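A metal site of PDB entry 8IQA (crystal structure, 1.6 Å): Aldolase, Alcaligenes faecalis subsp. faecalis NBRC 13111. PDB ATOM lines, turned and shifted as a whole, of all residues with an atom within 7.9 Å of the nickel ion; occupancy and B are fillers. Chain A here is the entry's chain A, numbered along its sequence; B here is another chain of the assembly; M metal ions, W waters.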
ATOM      1  N   LEU A  32      25.628  -3.509 -24.212  1.00  0.00           N
ATOM      2  CA  LEU A  32      26.278  -3.916 -22.935  1.00  0.00           C
ATOM      3  C   LEU A  32      26.963  -2.758 -22.222  1.00  0.00           C
ATOM      4  O   LEU A  32      27.694  -2.982 -21.266  1.00  0.00           O
ATOM      5  CB  LEU A  32      27.248  -5.098 -23.159  1.00  0.00           C
ATOM      6  CG  LEU A  32      26.601  -6.362 -23.731  1.00  0.00           C
ATOM      7  CD1 LEU A  32      27.634  -7.421 -24.053  1.00  0.00           C
ATOM      8  CD2 LEU A  32      25.527  -6.913 -22.789  1.00  0.00           C
ATOM      9  N   ALA A  33      26.652  -1.519 -22.584  1.00  0.00           N
ATOM     10  CA  ALA A  33      27.231  -0.343 -21.919  1.00  0.00           C
ATOM     11  C   ALA A  33      26.579  -0.079 -20.544  1.00  0.00           C
ATOM     12  O   ALA A  33      27.171   0.627 -19.729  1.00  0.00           O
ATOM     13  CB  ALA A  33      27.048   0.895 -22.814  1.00  0.00           C
ATOM     14  N   GLY A  34      25.365  -0.595 -20.314  1.00  0.00           N
ATOM     15  CA  GLY A  34      24.628  -0.336 -19.073  1.00  0.00           C
ATOM     16  C   GLY A  34      25.244  -0.908 -17.822  1.00  0.00           C
ATOM     17  O   GLY A  34      25.776  -2.029 -17.803  1.00  0.00           O
ATOM     18  N   GLN A  35      25.194  -0.123 -16.737  1.00  0.00           N
ATOM     19  CA  GLN A  35      25.742  -0.560 -15.440  1.00  0.00           C
ATOM     20  C   GLN A  35      24.727  -0.201 -14.352  1.00  0.00           C
ATOM     21  O   GLN A  35      24.126   0.882 -14.378  1.00  0.00           O
ATOM     22  CB  GLN A  35      27.000   0.195 -15.099  1.00  0.00           C
ATOM     23  CG  GLN A  35      28.177   0.044 -16.092  1.00  0.00           C
ATOM     24  CD  GLN A  35      29.271   1.036 -15.828  1.00  0.00           C
ATOM     25  OE1 GLN A  35      29.244   1.812 -14.883  1.00  0.00           O
ATOM     26  NE2 GLN A  35      30.266   1.077 -16.721  1.00  0.00           N
ATOM     27  N   ALA A  82      34.089  -2.528 -15.805  1.00  0.00           N
ATOM     28  CA  ALA A  82      33.826  -1.112 -15.941  1.00  0.00           C
ATOM     29  C   ALA A  82      32.993  -0.556 -14.764  1.00  0.00           C
ATOM     30  O   ALA A  82      32.877   0.658 -14.637  1.00  0.00           O
ATOM     31  CB  ALA A  82      33.133  -0.827 -17.280  1.00  0.00           C
ATOM     32  N   PHE A  85      34.620   1.591 -10.850  1.00  0.00           N
ATOM     33  CA  PHE A  85      34.646   3.012 -10.456  1.00  0.00           C
ATOM     34  C   PHE A  85      33.502   3.383  -9.518  1.00  0.00           C
ATOM     35  O   PHE A  85      33.623   4.390  -8.816  1.00  0.00           O
ATOM     36  CB  PHE A  85      34.689   3.937 -11.693  1.00  0.00           C
ATOM     37  CG  PHE A  85      33.358   4.286 -12.303  1.00  0.00           C
ATOM     38  CD1 PHE A  85      32.597   5.339 -11.815  1.00  0.00           C
ATOM     39  CD2 PHE A  85      32.836   3.526 -13.349  1.00  0.00           C
ATOM     40  CE1 PHE A  85      31.340   5.603 -12.335  1.00  0.00           C
ATOM     41  CE2 PHE A  85      31.605   3.840 -13.907  1.00  0.00           C
ATOM     42  CZ  PHE A  85      30.861   4.867 -13.383  1.00  0.00           C
ATOM     43  N   HIS A 101      24.441   3.783 -14.682  1.00  0.00           N
ATOM     44  CA  HIS A 101      25.136   4.491 -15.750  1.00  0.00           C
ATOM     45  C   HIS A 101      24.694   3.824 -17.051  1.00  0.00           C
ATOM     46  O   HIS A 101      24.780   2.592 -17.167  1.00  0.00           O
ATOM     47  CB  HIS A 101      26.665   4.407 -15.601  1.00  0.00           C
ATOM     48  CG  HIS A 101      27.404   4.768 -16.884  1.00  0.00           C
ATOM     49  ND1 HIS A 101      27.384   6.056 -17.403  1.00  0.00           N
ATOM     50  CD2 HIS A 101      28.187   3.993 -17.671  1.00  0.00           C
ATOM     51  CE1 HIS A 101      28.144   6.029 -18.488  1.00  0.00           C
ATOM     52  NE2 HIS A 101      28.629   4.805 -18.718  1.00  0.00           N
ATOM     53  N   THR A 102      24.202   4.596 -17.995  1.00  0.00           N
ATOM     54  CA  THR A 102      23.864   4.087 -19.337  1.00  0.00           C
ATOM     55  C   THR A 102      24.256   5.195 -20.385  1.00  0.00           C
ATOM     56  O   THR A 102      24.578   6.347 -20.043  1.00  0.00           O
ATOM     57  CB  THR A 102      22.374   3.634 -19.507  1.00  0.00           C
ATOM     58  OG1 THR A 102      21.567   4.790 -19.657  1.00  0.00           O
ATOM     59  CG2 THR A 102      21.830   2.815 -18.362  1.00  0.00           C
ATOM     60  N   HIS A 103      24.197   4.827 -21.656  1.00  0.00           N
ATOM     61  CA  HIS A 103      24.395   5.770 -22.757  1.00  0.00           C
ATOM     62  C   HIS A 103      23.003   5.793 -23.448  1.00  0.00           C
ATOM     63  O   HIS A 103      22.861   5.412 -24.609  1.00  0.00           O
ATOM     64  CB  HIS A 103      25.436   5.216 -23.751  1.00  0.00           C
ATOM     65  CG  HIS A 103      26.776   4.880 -23.174  1.00  0.00           C
ATOM     66  ND1 HIS A 103      27.758   4.291 -23.972  1.00  0.00           N
ATOM     67  CD2 HIS A 103      27.238   4.962 -21.897  1.00  0.00           C
ATOM     68  CE1 HIS A 103      28.789   4.091 -23.159  1.00  0.00           C
ATOM     69  NE2 HIS A 103      28.525   4.465 -21.904  1.00  0.00           N
ATOM     70  N   TRP A 137      36.202  14.534 -21.509  1.00  0.00           N
ATOM     71  CA  TRP A 137      36.037  13.121 -21.809  1.00  0.00           C
ATOM     72  C   TRP A 137      37.435  12.522 -21.734  1.00  0.00           C
ATOM     73  O   TRP A 137      38.305  12.862 -22.539  1.00  0.00           O
ATOM     74  CB  TRP A 137      35.449  12.910 -23.214  1.00  0.00           C
ATOM     75  CG  TRP A 137      35.288  11.468 -23.550  1.00  0.00           C
ATOM     76  CD1 TRP A 137      34.521  10.557 -22.878  1.00  0.00           C
ATOM     77  CD2 TRP A 137      35.903  10.757 -24.630  1.00  0.00           C
ATOM     78  NE1 TRP A 137      34.630   9.323 -23.470  1.00  0.00           N
ATOM     79  CE2 TRP A 137      35.455   9.421 -24.562  1.00  0.00           C
ATOM     80  CE3 TRP A 137      36.815  11.116 -25.630  1.00  0.00           C
ATOM     81  CZ2 TRP A 137      35.873   8.447 -25.466  1.00  0.00           C
ATOM     82  CZ3 TRP A 137      37.206  10.152 -26.547  1.00  0.00           C
ATOM     83  CH2 TRP A 137      36.721   8.835 -26.464  1.00  0.00           C
ATOM     84  N   GLU A 146      38.889   7.106 -13.558  1.00  0.00           N
ATOM     85  CA  GLU A 146      37.494   7.364 -13.852  1.00  0.00           C
ATOM     86  C   GLU A 146      36.696   7.664 -12.590  1.00  0.00           C
ATOM     87  O   GLU A 146      35.943   8.636 -12.555  1.00  0.00           O
ATOM     88  CB  GLU A 146      36.870   6.201 -14.643  1.00  0.00           C
ATOM     89  CG  GLU A 146      35.504   6.528 -15.210  1.00  0.00           C
ATOM     90  CD  GLU A 146      34.878   5.390 -15.985  1.00  0.00           C
ATOM     91  OE1 GLU A 146      35.227   4.222 -15.703  1.00  0.00           O
ATOM     92  OE2 GLU A 146      34.043   5.667 -16.893  1.00  0.00           O
ATOM     93  N   ILE A 150      34.886  11.218 -11.898  1.00  0.00           N
ATOM     94  CA  ILE A 150      33.428  11.252 -11.802  1.00  0.00           C
ATOM     95  C   ILE A 150      32.933  11.638 -10.398  1.00  0.00           C
ATOM     96  O   ILE A 150      32.017  12.449 -10.293  1.00  0.00           O
ATOM     97  CB  ILE A 150      32.803   9.931 -12.313  1.00  0.00           C
ATOM     98  CG1 ILE A 150      33.059   9.795 -13.851  1.00  0.00           C
ATOM     99  CG2 ILE A 150      31.294   9.856 -11.988  1.00  0.00           C
ATOM    100  CD1 ILE A 150      32.469   8.496 -14.486  1.00  0.00           C
ATOM    101  N   LEU A 162      27.830  13.143 -18.649  1.00  0.00           N
ATOM    102  CA  LEU A 162      29.252  12.945 -18.923  1.00  0.00           C
ATOM    103  C   LEU A 162      29.483  13.293 -20.380  1.00  0.00           C
ATOM    104  O   LEU A 162      29.059  12.525 -21.268  1.00  0.00           O
ATOM    105  CB  LEU A 162      29.573  11.467 -18.662  1.00  0.00           C
ATOM    106  CG  LEU A 162      29.226  10.986 -17.249  1.00  0.00           C
ATOM    107  CD1 LEU A 162      29.239   9.432 -17.153  1.00  0.00           C
ATOM    108  CD2 LEU A 162      30.199  11.572 -16.203  1.00  0.00           C
ATOM    109  N   HIS A 165      29.771  10.954 -23.733  1.00  0.00           N
ATOM    110  CA  HIS A 165      29.676   9.616 -23.150  1.00  0.00           C
ATOM    111  C   HIS A 165      28.265   9.179 -22.821  1.00  0.00           C
ATOM    112  O   HIS A 165      27.764   8.267 -23.485  1.00  0.00           O
ATOM    113  CB  HIS A 165      30.587   9.562 -21.919  1.00  0.00           C
ATOM    114  CG  HIS A 165      30.710   8.254 -21.229  1.00  0.00           C
ATOM    115  ND1 HIS A 165      31.529   8.122 -20.133  1.00  0.00           N
ATOM    116  CD2 HIS A 165      30.160   7.045 -21.512  1.00  0.00           C
ATOM    117  CE1 HIS A 165      31.441   6.850 -19.753  1.00  0.00           C
ATOM    118  NE2 HIS A 165      30.636   6.162 -20.551  1.00  0.00           N
ATOM    119  N   GLY A 166      27.647   9.743 -21.778  1.00  0.00           N
ATOM    120  CA  GLY A 166      26.313   9.306 -21.364  1.00  0.00           C
ATOM    121  C   GLY A 166      25.948   9.994 -20.075  1.00  0.00           C
ATOM    122  O   GLY A 166      26.186  11.196 -19.948  1.00  0.00           O
ATOM    123  N   TYR A 167      25.367   9.240 -19.125  1.00  0.00           N
ATOM    124  CA  TYR A 167      25.012   9.900 -17.842  1.00  0.00           C
ATOM    125  C   TYR A 167      25.187   8.903 -16.673  1.00  0.00           C
ATOM    126  O   TYR A 167      25.271   7.692 -16.884  1.00  0.00           O
ATOM    127  CB  TYR A 167      23.561  10.481 -17.897  1.00  0.00           C
ATOM    128  CG  TYR A 167      22.517   9.404 -17.688  1.00  0.00           C
ATOM    129  CD1 TYR A 167      22.177   8.978 -16.415  1.00  0.00           C
ATOM    130  CD2 TYR A 167      22.002   8.681 -18.760  1.00  0.00           C
ATOM    131  CE1 TYR A 167      21.420   7.831 -16.201  1.00  0.00           C
ATOM    132  CE2 TYR A 167      21.147   7.608 -18.562  1.00  0.00           C
ATOM    133  CZ  TYR A 167      20.890   7.147 -17.280  1.00  0.00           C
ATOM    134  OH  TYR A 167      20.075   6.050 -17.046  1.00  0.00           O
ATOM    135  N   GLN B 121      31.257  10.960 -29.548  1.00  0.00           N
ATOM    136  CA  GLN B 121      30.776  10.212 -28.412  1.00  0.00           C
ATOM    137  C   GLN B 121      31.406   8.823 -28.425  1.00  0.00           C
ATOM    138  O   GLN B 121      31.736   8.294 -29.488  1.00  0.00           O
ATOM    139  CB  GLN B 121      29.218  10.145 -28.476  1.00  0.00           C
ATOM    140  CG  GLN B 121      28.560   9.521 -27.248  1.00  0.00           C
ATOM    141  CD  GLN B 121      28.241   8.043 -27.393  1.00  0.00           C
ATOM    142  OE1 GLN B 121      28.305   7.491 -28.506  1.00  0.00           O
ATOM    143  NE2 GLN B 121      27.985   7.360 -26.267  1.00  0.00           N
ATOM    144  N   MET B 122      31.625   8.251 -27.233  1.00  0.00           N
ATOM    145  CA  MET B 122      32.249   6.947 -26.986  1.00  0.00           C
ATOM    146  C   MET B 122      31.823   5.852 -28.002  1.00  0.00           C
ATOM    147  O   MET B 122      32.694   5.190 -28.581  1.00  0.00           O
ATOM    148  CB  MET B 122      31.912   6.520 -25.552  1.00  0.00           C
ATOM    149  CG  MET B 122      32.286   5.081 -25.244  1.00  0.00           C
ATOM    150  SD  MET B 122      34.104   4.938 -25.162  1.00  0.00           S
ATOM    151  CE  MET B 122      34.241   3.211 -24.514  1.00  0.00           C
ATOM    152  N   ASP B 123      30.512   5.620 -28.159  1.00  0.00           N
ATOM    153  CA  ASP B 123      30.048   4.549 -29.049  1.00  0.00           C
ATOM    154  C   ASP B 123      30.216   4.844 -30.531  1.00  0.00           C
ATOM    155  O   ASP B 123      29.995   3.931 -31.344  1.00  0.00           O
ATOM    156  CB  ASP B 123      28.597   4.171 -28.732  1.00  0.00           C
ATOM    157  CG  ASP B 123      28.447   3.812 -27.259  1.00  0.00           C
ATOM    158  OD1 ASP B 123      29.306   3.038 -26.744  1.00  0.00           O
ATOM    159  OD2 ASP B 123      27.508   4.324 -26.629  1.00  0.00           O
HETATM  160 NI    NI M   1      29.830   4.280 -20.318  1.00  0.00          NI
HETATM  161  O   HOH W   1      31.491   3.572 -19.064  1.00  0.00           O
HETATM  162  O   HOH W   2      31.395   3.278 -21.608  1.00  0.00           O
HETATM  163  O   HOH W   3      29.358   2.039 -20.111  1.00  0.00           O
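The nickel ion is bound by NE2 of His 165, NE2 of His 103, NE2 of His 101, water W1, water W2 and water W3. The nickel ion has six donor atoms within binding distance.
The backbone carbonyl oxygen (O) of His 165 lies within hydrogen-bond range of the side-chain amide nitrogen (NE2) of Gln 121 of chain B, 2.9 Å away. A ring nitrogen (ND1) of His 103 is in hydrogen-bond range of the side-chain carboxylate of Asp 123 of chain B (2.7 Å). The backbone carbonyl oxygen (O) of His 101 lies within hydrogen-bond range of the backbone NH (N) of Gln 35. A ring nitrogen (ND1) of His 101 sits at hydrogen-bond distance from the backbone carbonyl oxygen (O) of Tyr 167 (2.7 Å).
Of the 19 residues printed, 3 come within 4 Å of the nickel ion. The nearest printed residue that does not touch the nickel ion is Ala 33 (4.6 Å).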
